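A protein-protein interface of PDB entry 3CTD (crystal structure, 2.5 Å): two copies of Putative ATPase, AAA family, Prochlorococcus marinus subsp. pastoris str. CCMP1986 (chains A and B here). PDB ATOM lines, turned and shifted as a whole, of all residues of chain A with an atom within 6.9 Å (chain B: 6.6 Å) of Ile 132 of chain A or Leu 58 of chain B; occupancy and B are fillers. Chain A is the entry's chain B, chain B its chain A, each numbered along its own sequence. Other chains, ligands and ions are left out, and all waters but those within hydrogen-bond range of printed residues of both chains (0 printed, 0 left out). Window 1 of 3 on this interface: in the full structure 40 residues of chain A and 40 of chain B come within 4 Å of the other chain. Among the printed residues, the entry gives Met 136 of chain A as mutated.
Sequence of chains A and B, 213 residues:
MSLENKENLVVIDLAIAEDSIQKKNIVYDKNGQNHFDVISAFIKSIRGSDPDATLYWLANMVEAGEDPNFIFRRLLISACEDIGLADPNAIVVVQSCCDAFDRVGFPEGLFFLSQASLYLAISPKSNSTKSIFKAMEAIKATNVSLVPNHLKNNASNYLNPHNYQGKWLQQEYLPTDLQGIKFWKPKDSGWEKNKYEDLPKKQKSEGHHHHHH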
ATOM      1  N   SER A 128     -18.067   3.658   6.985  1.00  0.00           N
ATOM      2  CA  SER A 128     -18.173   5.119   6.956  1.00  0.00           C
ATOM      3  C   SER A 128     -18.937   5.707   5.741  1.00  0.00           C
ATOM      4  O   SER A 128     -19.384   6.845   5.806  1.00  0.00           O
ATOM      5  CB  SER A 128     -16.827   5.814   7.193  1.00  0.00           C
ATOM      6  OG  SER A 128     -16.052   5.932   6.003  1.00  0.00           O
ATOM      7  N   THR A 129     -19.138   4.936   4.668  1.00  0.00           N
ATOM      8  CA  THR A 129     -19.945   5.425   3.563  1.00  0.00           C
ATOM      9  C   THR A 129     -21.414   5.474   3.893  1.00  0.00           C
ATOM     10  O   THR A 129     -22.171   6.035   3.097  1.00  0.00           O
ATOM     11  CB  THR A 129     -19.817   4.571   2.307  1.00  0.00           C
ATOM     12  OG1 THR A 129     -20.266   3.242   2.603  1.00  0.00           O
ATOM     13  CG2 THR A 129     -18.338   4.575   1.767  1.00  0.00           C
ATOM     14  N   LYS A 130     -21.824   4.877   5.023  1.00  0.00           N
ATOM     15  CA  LYS A 130     -23.248   4.943   5.476  1.00  0.00           C
ATOM     16  C   LYS A 130     -23.640   6.389   5.913  1.00  0.00           C
ATOM     17  O   LYS A 130     -24.814   6.716   6.050  1.00  0.00           O
ATOM     18  CB  LYS A 130     -23.573   3.912   6.602  1.00  0.00           C
ATOM     19  N   SER A 131     -22.626   7.221   6.117  1.00  0.00           N
ATOM     20  CA  SER A 131     -22.756   8.634   6.444  1.00  0.00           C
ATOM     21  C   SER A 131     -23.780   9.353   5.611  1.00  0.00           C
ATOM     22  O   SER A 131     -24.448  10.254   6.100  1.00  0.00           O
ATOM     23  CB  SER A 131     -21.429   9.314   6.200  1.00  0.00           C
ATOM     24  OG  SER A 131     -20.550   8.923   7.226  1.00  0.00           O
ATOM     25  N   ILE A 132     -23.872   8.985   4.339  1.00  0.00           N
ATOM     26  CA  ILE A 132     -24.732   9.703   3.411  1.00  0.00           C
ATOM     27  C   ILE A 132     -26.143   9.685   3.964  1.00  0.00           C
ATOM     28  O   ILE A 132     -26.882  10.625   3.762  1.00  0.00           O
ATOM     29  CB  ILE A 132     -24.687   9.078   1.976  1.00  0.00           C
ATOM     30  CG1 ILE A 132     -25.749   9.695   1.042  1.00  0.00           C
ATOM     31  CG2 ILE A 132     -24.939   7.605   2.073  1.00  0.00           C
ATOM     32  CD1 ILE A 132     -25.637  11.211   0.891  1.00  0.00           C
ATOM     33  N   PHE A 133     -26.517   8.613   4.652  1.00  0.00           N
ATOM     34  CA  PHE A 133     -27.865   8.515   5.239  1.00  0.00           C
ATOM     35  C   PHE A 133     -28.046   9.531   6.359  1.00  0.00           C
ATOM     36  O   PHE A 133     -29.148  10.032   6.578  1.00  0.00           O
ATOM     37  CB  PHE A 133     -28.152   7.110   5.765  1.00  0.00           C
ATOM     38  CG  PHE A 133     -28.144   6.057   4.705  1.00  0.00           C
ATOM     39  CD1 PHE A 133     -29.193   5.935   3.828  1.00  0.00           C
ATOM     40  CD2 PHE A 133     -27.086   5.174   4.593  1.00  0.00           C
ATOM     41  CE1 PHE A 133     -29.194   4.946   2.841  1.00  0.00           C
ATOM     42  CE2 PHE A 133     -27.067   4.192   3.592  1.00  0.00           C
ATOM     43  CZ  PHE A 133     -28.115   4.073   2.724  1.00  0.00           C
ATOM     44  N   LYS A 134     -26.970   9.833   7.079  1.00  0.00           N
ATOM     45  CA  LYS A 134     -27.063  10.839   8.125  1.00  0.00           C
ATOM     46  C   LYS A 134     -27.424  12.204   7.497  1.00  0.00           C
ATOM     47  O   LYS A 134     -28.399  12.842   7.892  1.00  0.00           O
ATOM     48  CB  LYS A 134     -25.755  10.910   8.950  1.00  0.00           C
ATOM     49  N   ALA A 135     -26.654  12.617   6.492  1.00  0.00           N
ATOM     50  CA  ALA A 135     -26.891  13.878   5.815  1.00  0.00           C
ATOM     51  C   ALA A 135     -28.266  13.895   5.151  1.00  0.00           C
ATOM     52  O   ALA A 135     -28.919  14.927   5.101  1.00  0.00           O
ATOM     53  CB  ALA A 135     -25.794  14.156   4.805  1.00  0.00           C
ATOM     54  N   MET A 136     -28.686  12.755   4.619  1.00  0.00           N
ATOM     55  CA  MET A 136     -30.004  12.617   4.058  1.00  0.00           C
ATOM     56  C   MET A 136     -31.080  12.881   5.131  1.00  0.00           C
ATOM     57  O   MET A 136     -32.172  13.376   4.823  1.00  0.00           O
ATOM     58  CB  MET A 136     -30.131  11.206   3.565  1.00  0.00           C
ATOM     59  CG  MET A 136     -31.219  10.968   2.616  1.00  0.00           C
ATOM     60  SD  MET A 136     -30.702   9.715   1.397  1.00  0.00           S
ATOM     61  CE  MET A 136     -30.080  10.821   0.113  1.00  0.00           C
ATOM     62  N   GLU A 137     -30.789  12.531   6.390  1.00  0.00           N
ATOM     63  CA  GLU A 137     -31.749  12.792   7.463  1.00  0.00           C
ATOM     64  C   GLU A 137     -31.773  14.266   7.848  1.00  0.00           C
ATOM     65  O   GLU A 137     -32.825  14.795   8.161  1.00  0.00           O
ATOM     66  CB  GLU A 137     -31.568  11.864   8.673  1.00  0.00           C
ATOM     67  CG  GLU A 137     -31.782  10.374   8.344  1.00  0.00           C
ATOM     68  CD  GLU A 137     -33.252  10.005   8.010  1.00  0.00           C
ATOM     69  OE1 GLU A 137     -34.161  10.388   8.792  1.00  0.00           O
ATOM     70  OE2 GLU A 137     -33.489   9.320   6.973  1.00  0.00           O
ATOM     71  N   ILE A 139     -31.357  16.588   5.573  1.00  0.00           N
ATOM     72  CA  ILE A 139     -32.062  17.219   4.465  1.00  0.00           C
ATOM     73  C   ILE A 139     -33.551  17.055   4.716  1.00  0.00           C
ATOM     74  O   ILE A 139     -34.322  17.989   4.541  1.00  0.00           O
ATOM     75  CB  ILE A 139     -31.710  16.557   3.098  1.00  0.00           C
ATOM     76  CG1 ILE A 139     -30.257  16.830   2.726  1.00  0.00           C
ATOM     77  CG2 ILE A 139     -32.679  16.970   1.998  1.00  0.00           C
ATOM     78  CD1 ILE A 139     -30.025  18.264   2.317  1.00  0.00           C
ATOM     79  N   PHE A 183     -21.066  14.858   9.516  1.00  0.00           N
ATOM     80  CA  PHE A 183     -21.742  13.658   9.016  1.00  0.00           C
ATOM     81  C   PHE A 183     -20.826  12.446   8.893  1.00  0.00           C
ATOM     82  O   PHE A 183     -21.261  11.313   9.109  1.00  0.00           O
ATOM     83  CB  PHE A 183     -22.417  13.919   7.680  1.00  0.00           C
ATOM     84  CG  PHE A 183     -23.485  14.970   7.740  1.00  0.00           C
ATOM     85  CD1 PHE A 183     -24.643  14.772   8.492  1.00  0.00           C
ATOM     86  CD2 PHE A 183     -23.334  16.162   7.048  1.00  0.00           C
ATOM     87  CE1 PHE A 183     -25.638  15.758   8.546  1.00  0.00           C
ATOM     88  CE2 PHE A 183     -24.299  17.128   7.086  1.00  0.00           C
ATOM     89  CZ  PHE A 183     -25.460  16.935   7.826  1.00  0.00           C
ATOM     90  N   VAL B  38     -26.817  23.287  -7.203  1.00  0.00           N
ATOM     91  CA  VAL B  38     -26.560  22.286  -6.175  1.00  0.00           C
ATOM     92  C   VAL B  38     -25.325  21.486  -6.541  1.00  0.00           C
ATOM     93  O   VAL B  38     -24.495  21.226  -5.677  1.00  0.00           O
ATOM     94  CB  VAL B  38     -27.738  21.323  -5.923  1.00  0.00           C
ATOM     95  CG1 VAL B  38     -27.354  20.346  -4.847  1.00  0.00           C
ATOM     96  CG2 VAL B  38     -28.986  22.102  -5.506  1.00  0.00           C
ATOM     97  N   PHE B  42     -21.810  21.039  -4.501  1.00  0.00           N
ATOM     98  CA  PHE B  42     -21.275  19.694  -4.329  1.00  0.00           C
ATOM     99  C   PHE B  42     -19.835  19.554  -4.819  1.00  0.00           C
ATOM    100  O   PHE B  42     -18.988  19.087  -4.054  1.00  0.00           O
ATOM    101  CB  PHE B  42     -22.207  18.711  -5.046  1.00  0.00           C
ATOM    102  CG  PHE B  42     -21.661  17.316  -5.217  1.00  0.00           C
ATOM    103  CD1 PHE B  42     -21.628  16.422  -4.154  1.00  0.00           C
ATOM    104  CD2 PHE B  42     -21.232  16.875  -6.469  1.00  0.00           C
ATOM    105  CE1 PHE B  42     -21.165  15.120  -4.325  1.00  0.00           C
ATOM    106  CE2 PHE B  42     -20.780  15.577  -6.644  1.00  0.00           C
ATOM    107  CZ  PHE B  42     -20.756  14.698  -5.575  1.00  0.00           C
ATOM    108  N   ALA B  53     -19.893  18.600   3.823  1.00  0.00           N
ATOM    109  CA  ALA B  53     -20.652  19.393   2.887  1.00  0.00           C
ATOM    110  C   ALA B  53     -20.878  18.581   1.621  1.00  0.00           C
ATOM    111  O   ALA B  53     -21.982  18.567   1.101  1.00  0.00           O
ATOM    112  CB  ALA B  53     -19.905  20.677   2.586  1.00  0.00           C
ATOM    113  N   THR B  54     -19.844  17.872   1.143  1.00  0.00           N
ATOM    114  CA  THR B  54     -20.010  16.961  -0.001  1.00  0.00           C
ATOM    115  C   THR B  54     -21.239  16.064   0.212  1.00  0.00           C
ATOM    116  O   THR B  54     -22.111  15.980  -0.657  1.00  0.00           O
ATOM    117  CB  THR B  54     -18.788  16.041  -0.199  1.00  0.00           C
ATOM    118  OG1 THR B  54     -17.635  16.809  -0.514  1.00  0.00           O
ATOM    119  CG2 THR B  54     -19.037  15.007  -1.281  1.00  0.00           C
ATOM    120  N   LEU B  55     -21.322  15.387   1.362  1.00  0.00           N
ATOM    121  CA  LEU B  55     -22.437  14.441   1.583  1.00  0.00           C
ATOM    122  C   LEU B  55     -23.732  15.220   1.627  1.00  0.00           C
ATOM    123  O   LEU B  55     -24.760  14.825   1.047  1.00  0.00           O
ATOM    124  CB  LEU B  55     -22.267  13.630   2.859  1.00  0.00           C
ATOM    125  CG  LEU B  55     -21.093  12.660   2.851  1.00  0.00           C
ATOM    126  CD1 LEU B  55     -20.842  12.236   4.225  1.00  0.00           C
ATOM    127  CD2 LEU B  55     -21.394  11.426   1.957  1.00  0.00           C
ATOM    128  N   TYR B  56     -23.667  16.368   2.272  1.00  0.00           N
ATOM    129  CA  TYR B  56     -24.862  17.171   2.383  1.00  0.00           C
ATOM    130  C   TYR B  56     -25.406  17.523   1.016  1.00  0.00           C
ATOM    131  O   TYR B  56     -26.576  17.225   0.738  1.00  0.00           O
ATOM    132  CB  TYR B  56     -24.615  18.404   3.230  1.00  0.00           C
ATOM    133  CG  TYR B  56     -25.810  19.263   3.351  1.00  0.00           C
ATOM    134  CD1 TYR B  56     -26.780  18.995   4.318  1.00  0.00           C
ATOM    135  CD2 TYR B  56     -25.963  20.381   2.506  1.00  0.00           C
ATOM    136  CE1 TYR B  56     -27.896  19.801   4.433  1.00  0.00           C
ATOM    137  CE2 TYR B  56     -27.071  21.164   2.571  1.00  0.00           C
ATOM    138  CZ  TYR B  56     -28.034  20.886   3.547  1.00  0.00           C
ATOM    139  OH  TYR B  56     -29.113  21.710   3.644  1.00  0.00           O
ATOM    140  N   TRP B  57     -24.588  18.124   0.144  1.00  0.00           N
ATOM    141  CA  TRP B  57     -25.085  18.411  -1.227  1.00  0.00           C
ATOM    142  C   TRP B  57     -25.443  17.131  -1.982  1.00  0.00           C
ATOM    143  O   TRP B  57     -26.453  17.094  -2.679  1.00  0.00           O
ATOM    144  CB  TRP B  57     -24.148  19.321  -2.026  1.00  0.00           C
ATOM    145  CG  TRP B  57     -23.946  20.632  -1.252  1.00  0.00           C
ATOM    146  CD1 TRP B  57     -22.790  21.075  -0.676  1.00  0.00           C
ATOM    147  CD2 TRP B  57     -24.960  21.618  -0.926  1.00  0.00           C
ATOM    148  NE1 TRP B  57     -23.010  22.275  -0.036  1.00  0.00           N
ATOM    149  CE2 TRP B  57     -24.331  22.627  -0.164  1.00  0.00           C
ATOM    150  CE3 TRP B  57     -26.332  21.726  -1.186  1.00  0.00           C
ATOM    151  CZ2 TRP B  57     -25.028  23.739   0.353  1.00  0.00           C
ATOM    152  CZ3 TRP B  57     -27.033  22.859  -0.687  1.00  0.00           C
ATOM    153  CH2 TRP B  57     -26.378  23.829   0.087  1.00  0.00           C
ATOM    154  N   LEU B  58     -24.648  16.074  -1.804  1.00  0.00           N
ATOM    155  CA  LEU B  58     -24.995  14.788  -2.407  1.00  0.00           C
ATOM    156  C   LEU B  58     -26.419  14.355  -2.022  1.00  0.00           C
ATOM    157  O   LEU B  58     -27.247  14.067  -2.906  1.00  0.00           O
ATOM    158  CB  LEU B  58     -23.950  13.690  -2.093  1.00  0.00           C
ATOM    159  CG  LEU B  58     -24.183  12.279  -2.662  1.00  0.00           C
ATOM    160  CD1 LEU B  58     -24.460  12.281  -4.154  1.00  0.00           C
ATOM    161  CD2 LEU B  58     -23.001  11.364  -2.286  1.00  0.00           C
ATOM    162  N   ALA B  59     -26.704  14.336  -0.722  1.00  0.00           N
ATOM    163  CA  ALA B  59     -28.059  13.967  -0.232  1.00  0.00           C
ATOM    164  C   ALA B  59     -29.112  14.862  -0.786  1.00  0.00           C
ATOM    165  O   ALA B  59     -30.170  14.402  -1.182  1.00  0.00           O
ATOM    166  CB  ALA B  59     -28.144  13.924   1.294  1.00  0.00           C
ATOM    167  N   ASN B  60     -28.823  16.147  -0.844  1.00  0.00           N
ATOM    168  CA  ASN B  60     -29.724  17.069  -1.514  1.00  0.00           C
ATOM    169  C   ASN B  60     -30.039  16.614  -2.951  1.00  0.00           C
ATOM    170  O   ASN B  60     -31.206  16.524  -3.350  1.00  0.00           O
ATOM    171  CB  ASN B  60     -29.132  18.477  -1.469  1.00  0.00           C
ATOM    172  CG  ASN B  60     -30.069  19.518  -1.998  1.00  0.00           C
ATOM    173  OD1 ASN B  60     -30.661  19.345  -3.073  1.00  0.00           O
ATOM    174  ND2 ASN B  60     -30.193  20.628  -1.276  1.00  0.00           N
ATOM    175  N   MET B  61     -29.020  16.252  -3.732  1.00  0.00           N
ATOM    176  CA  MET B  61     -29.313  15.892  -5.145  1.00  0.00           C
ATOM    177  C   MET B  61     -30.190  14.626  -5.245  1.00  0.00           C
ATOM    178  O   MET B  61     -31.090  14.560  -6.070  1.00  0.00           O
ATOM    179  CB  MET B  61     -28.041  15.785  -6.019  1.00  0.00           C
ATOM    180  CG  MET B  61     -27.254  17.081  -6.164  1.00  0.00           C
ATOM    181  SD  MET B  61     -25.870  17.039  -7.318  1.00  0.00           S
ATOM    182  CE  MET B  61     -24.706  16.102  -6.293  1.00  0.00           C
ATOM    183  N   VAL B  62     -29.952  13.641  -4.386  1.00  0.00           N
ATOM    184  CA  VAL B  62     -30.699  12.426  -4.506  1.00  0.00           C
ATOM    185  C   VAL B  62     -32.119  12.502  -3.906  1.00  0.00           C
ATOM    186  O   VAL B  62     -33.044  12.012  -4.501  1.00  0.00           O
ATOM    187  CB  VAL B  62     -29.923  11.141  -4.082  1.00  0.00           C
ATOM    188  CG1 VAL B  62     -28.423  11.356  -3.992  1.00  0.00           C
ATOM    189  CG2 VAL B  62     -30.518  10.535  -2.867  1.00  0.00           C
ATOM    190  N   GLU B  63     -32.319  13.192  -2.793  1.00  0.00           N
ATOM    191  CA  GLU B  63     -33.698  13.518  -2.420  1.00  0.00           C
ATOM    192  C   GLU B  63     -34.405  14.274  -3.541  1.00  0.00           C
ATOM    193  O   GLU B  63     -35.613  14.119  -3.712  1.00  0.00           O
ATOM    194  CB  GLU B  63     -33.794  14.331  -1.118  1.00  0.00           C
ATOM    195  CG  GLU B  63     -33.155  13.634   0.049  1.00  0.00           C
ATOM    196  CD  GLU B  63     -33.971  12.444   0.488  1.00  0.00           C
ATOM    197  OE1 GLU B  63     -35.161  12.646   0.813  1.00  0.00           O
ATOM    198  OE2 GLU B  63     -33.427  11.313   0.479  1.00  0.00           O
ATOM    199  N   ILE B  71     -24.510  12.970 -11.867  1.00  0.00           N
ATOM    200  CA  ILE B  71     -23.548  13.116 -10.759  1.00  0.00           C
ATOM    201  C   ILE B  71     -22.175  12.483 -11.113  1.00  0.00           C
ATOM    202  O   ILE B  71     -21.095  13.107 -10.921  1.00  0.00           O
ATOM    203  CB  ILE B  71     -24.142  12.587  -9.447  1.00  0.00           C
ATOM    204  CG1 ILE B  71     -25.434  13.366  -9.158  1.00  0.00           C
ATOM    205  CG2 ILE B  71     -23.095  12.643  -8.264  1.00  0.00           C
ATOM    206  CD1 ILE B  71     -26.423  12.702  -8.221  1.00  0.00           C
ATOM    207  N   LEU B  75     -18.216  13.698 -11.209  1.00  0.00           N
ATOM    208  CA  LEU B  75     -17.213  13.122 -10.336  1.00  0.00           C
ATOM    209  C   LEU B  75     -15.970  12.779 -11.161  1.00  0.00           C
ATOM    210  O   LEU B  75     -14.815  13.065 -10.761  1.00  0.00           O
ATOM    211  CB  LEU B  75     -17.770  11.886  -9.612  1.00  0.00           C
ATOM    212  CG  LEU B  75     -18.735  12.234  -8.454  1.00  0.00           C
ATOM    213  CD1 LEU B  75     -19.617  11.053  -7.970  1.00  0.00           C
ATOM    214  CD2 LEU B  75     -17.987  12.890  -7.284  1.00  0.00           C
ATOM    215  N   LEU B 110     -26.501   3.906  -3.960  1.00  0.00           N
ATOM    216  CA  LEU B 110     -26.163   5.071  -3.183  1.00  0.00           C
ATOM    217  C   LEU B 110     -24.755   4.934  -2.555  1.00  0.00           C
ATOM    218  O   LEU B 110     -24.035   5.915  -2.426  1.00  0.00           O
ATOM    219  CB  LEU B 110     -27.229   5.312  -2.087  1.00  0.00           C
ATOM    220  CG  LEU B 110     -27.089   6.576  -1.246  1.00  0.00           C
ATOM    221  CD1 LEU B 110     -26.860   7.804  -2.201  1.00  0.00           C
ATOM    222  CD2 LEU B 110     -28.318   6.787  -0.362  1.00  0.00           C
ATOM    223  N   PHE B 111     -24.377   3.726  -2.160  1.00  0.00           N
ATOM    224  CA  PHE B 111     -23.034   3.490  -1.639  1.00  0.00           C
ATOM    225  C   PHE B 111     -21.866   3.842  -2.617  1.00  0.00           C
ATOM    226  O   PHE B 111     -20.804   4.290  -2.178  1.00  0.00           O
ATOM    227  CB  PHE B 111     -22.921   2.044  -1.132  1.00  0.00           C
ATOM    228  CG  PHE B 111     -23.653   1.802   0.141  1.00  0.00           C
ATOM    229  CD1 PHE B 111     -23.232   2.436   1.335  1.00  0.00           C
ATOM    230  CD2 PHE B 111     -24.766   0.934   0.178  1.00  0.00           C
ATOM    231  CE1 PHE B 111     -23.921   2.222   2.559  1.00  0.00           C
ATOM    232  CE2 PHE B 111     -25.462   0.718   1.358  1.00  0.00           C
ATOM    233  CZ  PHE B 111     -25.048   1.360   2.569  1.00  0.00           C
ATOM    234  N   LEU B 113     -22.016   6.123  -4.936  1.00  0.00           N
ATOM    235  CA  LEU B 113     -22.101   7.541  -5.094  1.00  0.00           C
ATOM    236  C   LEU B 113     -21.384   8.130  -3.864  1.00  0.00           C
ATOM    237  O   LEU B 113     -20.544   9.035  -3.964  1.00  0.00           O
ATOM    238  CB  LEU B 113     -23.586   7.865  -5.149  1.00  0.00           C
ATOM    239  CG  LEU B 113     -24.374   8.666  -6.210  1.00  0.00           C
ATOM    240  CD1 LEU B 113     -23.637   9.073  -7.510  1.00  0.00           C
ATOM    241  CD2 LEU B 113     -25.771   8.030  -6.496  1.00  0.00           C
ATOM    242  N   SER B 114     -21.661   7.568  -2.701  1.00  0.00           N
ATOM    243  CA  SER B 114     -21.091   8.054  -1.470  1.00  0.00           C
ATOM    244  C   SER B 114     -19.605   7.734  -1.401  1.00  0.00           C
ATOM    245  O   SER B 114     -18.788   8.613  -1.009  1.00  0.00           O
ATOM    246  CB  SER B 114     -21.823   7.453  -0.262  1.00  0.00           C
ATOM    247  OG  SER B 114     -21.120   7.753   0.934  1.00  0.00           O
ATOM    248  N   GLN B 115     -19.207   6.515  -1.792  1.00  0.00           N
ATOM    249  CA  GLN B 115     -17.755   6.242  -1.737  1.00  0.00           C
ATOM    250  C   GLN B 115     -16.932   7.159  -2.686  1.00  0.00           C
ATOM    251  O   GLN B 115     -15.861   7.644  -2.363  1.00  0.00           O
ATOM    252  CB  GLN B 115     -17.414   4.748  -1.935  1.00  0.00           C
ATOM    253  CG  GLN B 115     -15.951   4.512  -2.478  1.00  0.00           C
ATOM    254  CD  GLN B 115     -15.411   3.162  -2.081  1.00  0.00           C
ATOM    255  OE1 GLN B 115     -15.981   2.510  -1.216  1.00  0.00           O
ATOM    256  NE2 GLN B 115     -14.321   2.730  -2.698  1.00  0.00           N
ATOM    257  N   SER B 117     -17.820   9.998  -3.881  1.00  0.00           N
ATOM    258  CA  SER B 117     -17.848  11.412  -3.452  1.00  0.00           C
ATOM    259  C   SER B 117     -16.927  11.638  -2.273  1.00  0.00           C
ATOM    260  O   SER B 117     -16.091  12.527  -2.319  1.00  0.00           O
ATOM    261  CB  SER B 117     -19.256  11.901  -3.131  1.00  0.00           C
ATOM    262  OG  SER B 117     -20.142  11.554  -4.195  1.00  0.00           O
ATOM    263  N   LEU B 118     -17.043  10.810  -1.237  1.00  0.00           N
ATOM    264  CA  LEU B 118     -16.113  10.909  -0.120  1.00  0.00           C
ATOM    265  C   LEU B 118     -14.666  10.699  -0.551  1.00  0.00           C
ATOM    266  O   LEU B 118     -13.740  11.320  -0.027  1.00  0.00           O
ATOM    267  CB  LEU B 118     -16.469   9.897   0.983  1.00  0.00           C
ATOM    268  CG  LEU B 118     -17.746  10.222   1.758  1.00  0.00           C
ATOM    269  CD1 LEU B 118     -18.295   8.972   2.424  1.00  0.00           C
ATOM    270  CD2 LEU B 118     -17.483  11.319   2.769  1.00  0.00           C
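The backbone carbonyl oxygen (O) of Phe 183 of chain A lies within hydrogen-bond range of the side-chain hydroxyl (OG) of Ser 131 of chain A (3.1 Å).
The backbone carbonyl oxygen (O) of Ser 128 of chain A lies within hydrogen-bond range of the side-chain hydroxyl (OG) of Ser 131 of chain A, at 2.8 Å.
No position is printed for both chains.
Of the 12 printed residues of chain A, 7 touch a printed residue of chain B.
Of the 22 printed residues of chain B, 11 touch a printed residue of chain A.
Hydrophobic or aromatic side chains of chain B within 4 Å of the printed part of chain A: Leu 55, Tyr 56, Leu 58, Ala 59, Val 62, Leu 110 and Phe 111.
Leu 55 of chain B touches Ser 131 of chain A.
CD1 of Ile 132 of chain A touches O of Leu 55 of chain B, 3.7 Å away.
Ile 132 of chain A touches Leu 58 of chain B (CD1 to CG, 3.98 Å).
N of Ala 59 of chain B touches CD1 of Ile 132 of chain A (3.7 Å).
Ile 132 of chain A touches Leu 110 of chain B.
Ile 132 of chain A touches Ser 114 of chain B (CG2 to CB, 3.9 Å).
Phe 133 of chain A touches Phe 111 of chain B (CE2 to CZ, 3.6 Å).
Ala 59 of chain B touches Met 136 of chain A (CB to N, 3.6 Å).
CE of Met 136 of chain A touches CG2 of Val 62 of chain B (3.0 Å).
CD1 of Ile 139 of chain A touches CB of Asn 60 of chain B, at 3.9 Å.
The side-chain hydroxyl (OG) of Ser 114 of chain B is in hydrogen-bond range of the backbone carbonyl oxygen (O) of Thr 129 of chain A (3.0 Å).
The side-chain sulfur (SD) of Met 136 of chain A sits close to the side-chain carboxylate (OE2) of Glu 63 of chain B, at 3.3 Å.
Of the printed residues of chain B, Ile 132 of chain A touches Leu 55, Leu 58, Ala 59, Leu 110 and Ser 114.
Of the printed residues of chain A, Leu 58 of chain B touches Ile 132 (3.98 Å).
Of the printed residues of chain A, Asn 60 of chain B touches Ile 139 (3.9 Å).
Of the printed residues of chain A, Val 62 of chain B touches Met 136 (3.0 Å).
Val 38 of chain B touches none of the printed residues of chain A.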
